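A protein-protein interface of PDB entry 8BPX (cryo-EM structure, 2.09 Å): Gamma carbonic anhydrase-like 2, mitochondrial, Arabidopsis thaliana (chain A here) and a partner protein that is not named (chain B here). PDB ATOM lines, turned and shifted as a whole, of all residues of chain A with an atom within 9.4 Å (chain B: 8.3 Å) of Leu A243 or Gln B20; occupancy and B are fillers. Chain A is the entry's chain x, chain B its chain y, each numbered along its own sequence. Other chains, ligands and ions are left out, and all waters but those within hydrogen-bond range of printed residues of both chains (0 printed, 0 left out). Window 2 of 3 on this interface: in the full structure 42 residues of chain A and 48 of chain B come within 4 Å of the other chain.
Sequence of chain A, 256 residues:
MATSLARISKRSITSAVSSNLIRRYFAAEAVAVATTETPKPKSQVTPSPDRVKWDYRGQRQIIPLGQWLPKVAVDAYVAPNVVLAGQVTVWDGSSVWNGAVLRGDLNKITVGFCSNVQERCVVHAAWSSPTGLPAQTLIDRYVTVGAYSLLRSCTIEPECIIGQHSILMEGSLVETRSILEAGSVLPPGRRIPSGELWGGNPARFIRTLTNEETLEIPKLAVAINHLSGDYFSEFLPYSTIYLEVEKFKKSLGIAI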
ATOM      1  N   SER A 239       4.707  25.394  25.029  1.00  0.00           N
ATOM      2  CA  SER A 239       4.819  24.727  23.744  1.00  0.00           C
ATOM      3  C   SER A 239       6.277  24.721  23.282  1.00  0.00           C
ATOM      4  O   SER A 239       7.132  25.419  23.826  1.00  0.00           O
ATOM      5  CB  SER A 239       3.933  25.418  22.707  1.00  0.00           C
ATOM      6  OG  SER A 239       3.820  24.624  21.541  1.00  0.00           O
ATOM      7  N   THR A 240       6.555  23.917  22.258  1.00  0.00           N
ATOM      8  CA  THR A 240       7.878  23.868  21.648  1.00  0.00           C
ATOM      9  C   THR A 240       7.928  24.597  20.307  1.00  0.00           C
ATOM     10  O   THR A 240       8.860  24.376  19.527  1.00  0.00           O
ATOM     11  CB  THR A 240       8.338  22.417  21.481  1.00  0.00           C
ATOM     12  OG1 THR A 240       7.276  21.632  20.925  1.00  0.00           O
ATOM     13  CG2 THR A 240       8.749  21.830  22.818  1.00  0.00           C
ATOM     14  N   ILE A 241       6.949  25.463  20.031  1.00  0.00           N
ATOM     15  CA  ILE A 241       6.922  26.194  18.764  1.00  0.00           C
ATOM     16  C   ILE A 241       8.119  27.128  18.654  1.00  0.00           C
ATOM     17  O   ILE A 241       8.667  27.330  17.563  1.00  0.00           O
ATOM     18  CB  ILE A 241       5.602  26.970  18.616  1.00  0.00           C
ATOM     19  CG1 ILE A 241       4.421  26.032  18.790  1.00  0.00           C
ATOM     20  CG2 ILE A 241       5.518  27.621  17.250  1.00  0.00           C
ATOM     21  CD1 ILE A 241       4.472  24.923  17.834  1.00  0.00           C
ATOM     22  N   TYR A 242       8.534  27.720  19.776  1.00  0.00           N
ATOM     23  CA  TYR A 242       9.640  28.672  19.744  1.00  0.00           C
ATOM     24  C   TYR A 242      10.898  28.056  19.142  1.00  0.00           C
ATOM     25  O   TYR A 242      11.681  28.761  18.504  1.00  0.00           O
ATOM     26  CB  TYR A 242       9.901  29.221  21.149  1.00  0.00           C
ATOM     27  CG  TYR A 242      10.548  28.259  22.122  1.00  0.00           C
ATOM     28  CD1 TYR A 242       9.777  27.400  22.893  1.00  0.00           C
ATOM     29  CD2 TYR A 242      11.926  28.231  22.295  1.00  0.00           C
ATOM     30  CE1 TYR A 242      10.360  26.529  23.795  1.00  0.00           C
ATOM     31  CE2 TYR A 242      12.520  27.364  23.196  1.00  0.00           C
ATOM     32  CZ  TYR A 242      11.731  26.516  23.942  1.00  0.00           C
ATOM     33  OH  TYR A 242      12.317  25.648  24.837  1.00  0.00           O
ATOM     34  N   LEU A 243      11.091  26.745  19.304  1.00  0.00           N
ATOM     35  CA  LEU A 243      12.200  26.068  18.634  1.00  0.00           C
ATOM     36  C   LEU A 243      12.053  26.125  17.116  1.00  0.00           C
ATOM     37  O   LEU A 243      13.034  26.353  16.393  1.00  0.00           O
ATOM     38  CB  LEU A 243      12.275  24.617  19.102  1.00  0.00           C
ATOM     39  CG  LEU A 243      12.851  24.357  20.493  1.00  0.00           C
ATOM     40  CD1 LEU A 243      13.264  22.902  20.613  1.00  0.00           C
ATOM     41  CD2 LEU A 243      14.026  25.281  20.759  1.00  0.00           C
ATOM     42  N   GLU A 244      10.834  25.893  16.618  1.00  0.00           N
ATOM     43  CA  GLU A 244      10.578  25.987  15.186  1.00  0.00           C
ATOM     44  C   GLU A 244      10.829  27.398  14.683  1.00  0.00           C
ATOM     45  O   GLU A 244      11.413  27.591  13.610  1.00  0.00           O
ATOM     46  CB  GLU A 244       9.138  25.567  14.878  1.00  0.00           C
ATOM     47  CG  GLU A 244       8.720  24.101  15.134  1.00  0.00           C
ATOM     48  CD  GLU A 244       9.750  23.014  14.810  1.00  0.00           C
ATOM     49  OE1 GLU A 244      10.866  23.295  14.333  1.00  0.00           O
ATOM     50  OE2 GLU A 244       9.424  21.830  15.046  1.00  0.00           O
ATOM     51  N   VAL A 245      10.385  28.396  15.445  1.00  0.00           N
ATOM     52  CA  VAL A 245      10.662  29.786  15.099  1.00  0.00           C
ATOM     53  C   VAL A 245      12.165  30.032  15.051  1.00  0.00           C
ATOM     54  O   VAL A 245      12.666  30.726  14.160  1.00  0.00           O
ATOM     55  CB  VAL A 245       9.962  30.732  16.093  1.00  0.00           C
ATOM     56  CG1 VAL A 245      10.111  32.176  15.650  1.00  0.00           C
ATOM     57  CG2 VAL A 245       8.494  30.366  16.233  1.00  0.00           C
ATOM     58  N   GLU A 246      12.905  29.458  16.004  1.00  0.00           N
ATOM     59  CA  GLU A 246      14.355  29.630  16.043  1.00  0.00           C
ATOM     60  C   GLU A 246      15.012  29.088  14.779  1.00  0.00           C
ATOM     61  O   GLU A 246      15.858  29.753  14.171  1.00  0.00           O
ATOM     62  CB  GLU A 246      14.935  28.930  17.271  1.00  0.00           C
ATOM     63  CG  GLU A 246      16.247  29.502  17.751  1.00  0.00           C
ATOM     64  CD  GLU A 246      16.812  28.751  18.942  1.00  0.00           C
ATOM     65  OE1 GLU A 246      16.043  28.035  19.620  1.00  0.00           O
ATOM     66  OE2 GLU A 246      18.026  28.879  19.200  1.00  0.00           O
ATOM     67  N   LYS A 247      14.647  27.870  14.374  1.00  0.00           N
ATOM     68  CA  LYS A 247      15.313  27.302  13.202  1.00  0.00           C
ATOM     69  C   LYS A 247      14.845  27.978  11.915  1.00  0.00           C
ATOM     70  O   LYS A 247      15.629  28.133  10.971  1.00  0.00           O
ATOM     71  CB  LYS A 247      15.118  25.788  13.123  1.00  0.00           C
ATOM     72  CG  LYS A 247      13.795  25.258  13.583  1.00  0.00           C
ATOM     73  CD  LYS A 247      13.649  23.817  13.140  1.00  0.00           C
ATOM     74  CE  LYS A 247      14.535  22.893  13.963  1.00  0.00           C
ATOM     75  NZ  LYS A 247      14.489  23.216  15.415  1.00  0.00           N
ATOM     76  N   PHE A 248      13.576  28.394  11.861  1.00  0.00           N
ATOM     77  CA  PHE A 248      13.093  29.178  10.729  1.00  0.00           C
ATOM     78  C   PHE A 248      13.877  30.477  10.598  1.00  0.00           C
ATOM     79  O   PHE A 248      14.172  30.924   9.486  1.00  0.00           O
ATOM     80  CB  PHE A 248      11.598  29.459  10.902  1.00  0.00           C
ATOM     81  CG  PHE A 248      10.887  29.851   9.634  1.00  0.00           C
ATOM     82  CD1 PHE A 248      10.932  31.153   9.170  1.00  0.00           C
ATOM     83  CD2 PHE A 248      10.148  28.919   8.921  1.00  0.00           C
ATOM     84  CE1 PHE A 248      10.267  31.517   8.010  1.00  0.00           C
ATOM     85  CE2 PHE A 248       9.482  29.279   7.761  1.00  0.00           C
ATOM     86  CZ  PHE A 248       9.544  30.579   7.306  1.00  0.00           C
ATOM     87  N   LYS A 249      14.212  31.100  11.728  1.00  0.00           N
ATOM     88  CA  LYS A 249      15.044  32.297  11.714  1.00  0.00           C
ATOM     89  C   LYS A 249      16.457  31.979  11.243  1.00  0.00           C
ATOM     90  O   LYS A 249      17.029  32.706  10.423  1.00  0.00           O
ATOM     91  CB  LYS A 249      15.082  32.914  13.110  1.00  0.00           C
ATOM     92  CG  LYS A 249      13.981  33.902  13.405  1.00  0.00           C
ATOM     93  CD  LYS A 249      14.308  34.678  14.659  1.00  0.00           C
ATOM     94  CE  LYS A 249      13.255  34.463  15.728  1.00  0.00           C
ATOM     95  NZ  LYS A 249      12.058  35.297  15.492  1.00  0.00           N
ATOM     96  N   LYS A 250      17.040  30.898  11.768  1.00  0.00           N
ATOM     97  CA  LYS A 250      18.424  30.565  11.440  1.00  0.00           C
ATOM     98  C   LYS A 250      18.582  30.260   9.957  1.00  0.00           C
ATOM     99  O   LYS A 250      19.571  30.661   9.334  1.00  0.00           O
ATOM    100  CB  LYS A 250      18.896  29.384  12.283  1.00  0.00           C
ATOM    101  CG  LYS A 250      19.189  29.730  13.730  1.00  0.00           C
ATOM    102  CD  LYS A 250      19.405  28.472  14.557  1.00  0.00           C
ATOM    103  CE  LYS A 250      19.705  28.802  16.008  1.00  0.00           C
ATOM    104  NZ  LYS A 250      19.561  27.607  16.885  1.00  0.00           N
ATOM    105  N   SER A 251      17.608  29.559   9.371  1.00  0.00           N
ATOM    106  CA  SER A 251      17.643  29.283   7.940  1.00  0.00           C
ATOM    107  C   SER A 251      17.570  30.552   7.103  1.00  0.00           C
ATOM    108  O   SER A 251      17.869  30.506   5.905  1.00  0.00           O
ATOM    109  CB  SER A 251      16.495  28.345   7.562  1.00  0.00           C
ATOM    110  OG  SER A 251      15.268  29.047   7.506  1.00  0.00           O
ATOM    111  N   GLY B  12      25.231  26.810  28.975  1.00  0.00           N
ATOM    112  CA  GLY B  12      23.844  26.880  28.547  1.00  0.00           C
ATOM    113  C   GLY B  12      23.579  26.048  27.309  1.00  0.00           C
ATOM    114  O   GLY B  12      22.530  25.413  27.189  1.00  0.00           O
ATOM    115  N   ASN B  13      24.531  26.031  26.374  1.00  0.00           N
ATOM    116  CA  ASN B  13      24.404  25.170  25.200  1.00  0.00           C
ATOM    117  C   ASN B  13      24.314  23.702  25.604  1.00  0.00           C
ATOM    118  O   ASN B  13      23.475  22.950  25.090  1.00  0.00           O
ATOM    119  CB  ASN B  13      25.586  25.393  24.258  1.00  0.00           C
ATOM    120  CG  ASN B  13      25.269  26.351  23.135  1.00  0.00           C
ATOM    121  OD1 ASN B  13      24.138  26.806  22.991  1.00  0.00           O
ATOM    122  ND2 ASN B  13      26.274  26.669  22.334  1.00  0.00           N
ATOM    123  N   TRP B  14      25.178  23.280  26.531  1.00  0.00           N
ATOM    124  CA  TRP B  14      25.131  21.897  27.008  1.00  0.00           C
ATOM    125  C   TRP B  14      23.787  21.577  27.655  1.00  0.00           C
ATOM    126  O   TRP B  14      23.204  20.510  27.414  1.00  0.00           O
ATOM    127  CB  TRP B  14      26.256  21.637  28.009  1.00  0.00           C
ATOM    128  CG  TRP B  14      27.631  21.713  27.444  1.00  0.00           C
ATOM    129  CD1 TRP B  14      27.982  21.714  26.129  1.00  0.00           C
ATOM    130  CD2 TRP B  14      28.849  21.811  28.185  1.00  0.00           C
ATOM    131  NE1 TRP B  14      29.346  21.799  26.005  1.00  0.00           N
ATOM    132  CE2 TRP B  14      29.902  21.861  27.255  1.00  0.00           C
ATOM    133  CE3 TRP B  14      29.152  21.858  29.550  1.00  0.00           C
ATOM    134  CZ2 TRP B  14      31.233  21.957  27.642  1.00  0.00           C
ATOM    135  CZ3 TRP B  14      30.470  21.954  29.932  1.00  0.00           C
ATOM    136  CH2 TRP B  14      31.497  22.002  28.982  1.00  0.00           C
ATOM    137  N   ILE B  15      23.291  22.490  28.492  1.00  0.00           N
ATOM    138  CA  ILE B  15      22.019  22.271  29.175  1.00  0.00           C
ATOM    139  C   ILE B  15      20.877  22.185  28.168  1.00  0.00           C
ATOM    140  O   ILE B  15      19.962  21.368  28.316  1.00  0.00           O
ATOM    141  CB  ILE B  15      21.782  23.373  30.225  1.00  0.00           C
ATOM    142  CG1 ILE B  15      22.846  23.292  31.320  1.00  0.00           C
ATOM    143  CG2 ILE B  15      20.389  23.260  30.828  1.00  0.00           C
ATOM    144  CD1 ILE B  15      22.667  24.302  32.421  1.00  0.00           C
ATOM    145  N   ARG B  16      20.916  23.019  27.128  1.00  0.00           N
ATOM    146  CA  ARG B  16      19.887  22.968  26.093  1.00  0.00           C
ATOM    147  C   ARG B  16      19.915  21.642  25.344  1.00  0.00           C
ATOM    148  O   ARG B  16      18.862  21.047  25.075  1.00  0.00           O
ATOM    149  CB  ARG B  16      20.070  24.129  25.121  1.00  0.00           C
ATOM    150  CG  ARG B  16      19.769  25.485  25.718  1.00  0.00           C
ATOM    151  CD  ARG B  16      19.499  26.491  24.631  1.00  0.00           C
ATOM    152  NE  ARG B  16      18.300  26.138  23.884  1.00  0.00           N
ATOM    153  CZ  ARG B  16      17.969  26.652  22.710  1.00  0.00           C
ATOM    154  NH1 ARG B  16      18.729  27.553  22.112  1.00  0.00           N
ATOM    155  NH2 ARG B  16      16.843  26.257  22.125  1.00  0.00           N
ATOM    156  N   GLY B  17      21.111  21.172  24.983  1.00  0.00           N
ATOM    157  CA  GLY B  17      21.211  19.875  24.334  1.00  0.00           C
ATOM    158  C   GLY B  17      20.643  18.763  25.193  1.00  0.00           C
ATOM    159  O   GLY B  17      19.870  17.923  24.719  1.00  0.00           O
ATOM    160  N   THR B  18      20.993  18.766  26.484  1.00  0.00           N
ATOM    161  CA  THR B  18      20.463  17.754  27.393  1.00  0.00           C
ATOM    162  C   THR B  18      18.943  17.836  27.493  1.00  0.00           C
ATOM    163  O   THR B  18      18.256  16.807  27.497  1.00  0.00           O
ATOM    164  CB  THR B  18      21.091  17.900  28.780  1.00  0.00           C
ATOM    165  OG1 THR B  18      22.518  17.861  28.671  1.00  0.00           O
ATOM    166  CG2 THR B  18      20.620  16.783  29.699  1.00  0.00           C
ATOM    167  N   GLY B  19      18.400  19.051  27.585  1.00  0.00           N
ATOM    168  CA  GLY B  19      16.959  19.195  27.702  1.00  0.00           C
ATOM    169  C   GLY B  19      16.218  18.691  26.479  1.00  0.00           C
ATOM    170  O   GLY B  19      15.198  18.007  26.597  1.00  0.00           O
ATOM    171  N   GLN B  20      16.721  19.018  25.288  1.00  0.00           N
ATOM    172  CA  GLN B  20      16.069  18.530  24.077  1.00  0.00           C
ATOM    173  C   GLN B  20      16.208  17.014  23.934  1.00  0.00           C
ATOM    174  O   GLN B  20      15.277  16.350  23.454  1.00  0.00           O
ATOM    175  CB  GLN B  20      16.620  19.272  22.858  1.00  0.00           C
ATOM    176  CG  GLN B  20      16.396  20.783  22.947  1.00  0.00           C
ATOM    177  CD  GLN B  20      16.634  21.514  21.643  1.00  0.00           C
ATOM    178  OE1 GLN B  20      16.343  21.001  20.564  1.00  0.00           O
ATOM    179  NE2 GLN B  20      17.157  22.730  21.737  1.00  0.00           N
ATOM    180  N   ALA B  21      17.330  16.441  24.380  1.00  0.00           N
ATOM    181  CA  ALA B  21      17.449  14.984  24.392  1.00  0.00           C
ATOM    182  C   ALA B  21      16.425  14.351  25.331  1.00  0.00           C
ATOM    183  O   ALA B  21      15.806  13.335  24.993  1.00  0.00           O
ATOM    184  CB  ALA B  21      18.867  14.572  24.784  1.00  0.00           C
ATOM    185  N   LEU B  22      16.237  14.938  26.516  1.00  0.00           N
ATOM    186  CA  LEU B  22      15.233  14.427  27.444  1.00  0.00           C
ATOM    187  C   LEU B  22      13.834  14.535  26.853  1.00  0.00           C
ATOM    188  O   LEU B  22      13.002  13.640  27.040  1.00  0.00           O
ATOM    189  CB  LEU B  22      15.307  15.172  28.777  1.00  0.00           C
ATOM    190  CG  LEU B  22      16.351  14.684  29.782  1.00  0.00           C
ATOM    191  CD1 LEU B  22      16.199  15.408  31.112  1.00  0.00           C
ATOM    192  CD2 LEU B  22      16.235  13.185  29.978  1.00  0.00           C
ATOM    193  N   ASP B  23      13.551  15.631  26.145  1.00  0.00           N
ATOM    194  CA  ASP B  23      12.250  15.771  25.499  1.00  0.00           C
ATOM    195  C   ASP B  23      12.040  14.687  24.447  1.00  0.00           C
ATOM    196  O   ASP B  23      10.951  14.108  24.350  1.00  0.00           O
ATOM    197  CB  ASP B  23      12.114  17.163  24.879  1.00  0.00           C
ATOM    198  CG  ASP B  23      10.673  17.523  24.545  1.00  0.00           C
ATOM    199  OD1 ASP B  23       9.751  17.023  25.219  1.00  0.00           O
ATOM    200  OD2 ASP B  23      10.458  18.312  23.603  1.00  0.00           O
ATOM    201  N   ARG B  24      13.076  14.385  23.658  1.00  0.00           N
ATOM    202  CA  ARG B  24      12.955  13.317  22.668  1.00  0.00           C
ATOM    203  C   ARG B  24      12.725  11.962  23.332  1.00  0.00           C
ATOM    204  O   ARG B  24      11.898  11.167  22.869  1.00  0.00           O
ATOM    205  CB  ARG B  24      14.194  13.273  21.774  1.00  0.00           C
ATOM    206  CG  ARG B  24      14.128  14.239  20.612  1.00  0.00           C
ATOM    207  CD  ARG B  24      15.445  14.345  19.853  1.00  0.00           C
ATOM    208  NE  ARG B  24      16.610  13.979  20.647  1.00  0.00           N
ATOM    209  CZ  ARG B  24      17.669  14.756  20.821  1.00  0.00           C
ATOM    210  NH1 ARG B  24      17.720  15.979  20.317  1.00  0.00           N
ATOM    211  NH2 ARG B  24      18.709  14.294  21.510  1.00  0.00           N
ATOM    212  N   VAL B  25      13.445  11.682  24.420  1.00  0.00           N
ATOM    213  CA  VAL B  25      13.253  10.417  25.128  1.00  0.00           C
ATOM    214  C   VAL B  25      11.829  10.317  25.666  1.00  0.00           C
ATOM    215  O   VAL B  25      11.184   9.263  25.574  1.00  0.00           O
ATOM    216  CB  VAL B  25      14.301  10.263  26.248  1.00  0.00           C
ATOM    217  CG1 VAL B  25      13.952   9.086  27.141  1.00  0.00           C
ATOM    218  CG2 VAL B  25      15.686  10.084  25.649  1.00  0.00           C
ATOM    219  N   GLY B  26      11.316  11.410  26.233  1.00  0.00           N
ATOM    220  CA  GLY B  26       9.948  11.405  26.725  1.00  0.00           C
ATOM    221  C   GLY B  26       8.930  11.206  25.619  1.00  0.00           C
ATOM    222  O   GLY B  26       7.915  10.532  25.810  1.00  0.00           O
ATOM    223  N   SER B  27       9.182  11.793  24.448  1.00  0.00           N
ATOM    224  CA  SER B  27       8.308  11.563  23.304  1.00  0.00           C
ATOM    225  C   SER B  27       8.325  10.098  22.884  1.00  0.00           C
ATOM    226  O   SER B  27       7.280   9.528  22.554  1.00  0.00           O
ATOM    227  CB  SER B  27       8.716  12.461  22.140  1.00  0.00           C
ATOM    228  OG  SER B  27       8.622  13.828  22.497  1.00  0.00           O
ATOM    229  N   LEU B  39       4.581  25.419  13.565  1.00  0.00           N
ATOM    230  CA  LEU B  39       4.419  26.805  13.148  1.00  0.00           C
ATOM    231  C   LEU B  39       3.065  27.000  12.478  1.00  0.00           C
ATOM    232  O   LEU B  39       2.605  26.149  11.712  1.00  0.00           O
ATOM    233  CB  LEU B  39       5.541  27.192  12.188  1.00  0.00           C
ATOM    234  CG  LEU B  39       5.951  28.660  12.142  1.00  0.00           C
ATOM    235  CD1 LEU B  39       6.256  29.178  13.535  1.00  0.00           C
ATOM    236  CD2 LEU B  39       7.136  28.838  11.220  1.00  0.00           C
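The backbone carbonyl oxygen (O) of Phe A248 sits at hydrogen-bond distance from the side-chain hydroxyl (OG) of Ser A251.
The side-chain carboxylate (OE2) of Glu A246 lies within salt-bridge range of the side-chain amino group (NZ) of Lys A250, at 3.1 Å.
O of Asp B23 is in hydrogen-bond range of OG of Ser B27.
Of the 13 printed residues of chain A, 5 touch a printed residue of chain B.
Hydrophobic or aromatic side chains of chain A within 4 Å of the printed part of chain B: Leu A243, Val A245 and Phe A248.
Of the 17 printed residues of chain B, 4 touch a printed residue of chain A.
Hydrophobic or aromatic side chains of chain B that line the printed part of chain A: Leu B39.
Among the printed residues, 6 pairs touch across the chains.
OE1 of Glu A246 lies within salt-bridge range of NH2 of Arg B16, at 3.2 Å.
Leu A243 touches two residues of chain B.
Of chain A, only Leu A243 (3.6 Å) comes within 4 Å of Gln B20.
No residue of chain A comes within 4 Å of Gly B17.
No residue of chain A comes within 4 Å of Gly B19.
No residue of chain A comes within 4 Å of Ala B21.
Of the printed residues of chain B, Phe A248 touches Leu B39.
Of the printed residues of chain B, Glu A246 touches Arg B16 (3.2 Å).
Of the printed residues of chain B, Val A245 touches Leu B39.
Trp B14 touches none of the printed residues of chain A.
Gly B26 touches none of the printed residues of chain A.
The nearest residue of chain B that does not touch Leu A243 is Asp B23 (6.2 Å).
The nearest residue of chain A that does not touch Gln B20 is Glu A246 (5.8 Å).
The nearest printed residue of chain A that does not touch Arg B16 is Tyr A242 (4.6 Å).
Among the printed residues, merely in contact across the chains: Thr A240 with Asp B23, Leu A243 with Arg B16, Leu A243 with Gln B20, Val A245 with Leu B39 and Phe A248 with Leu B39.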
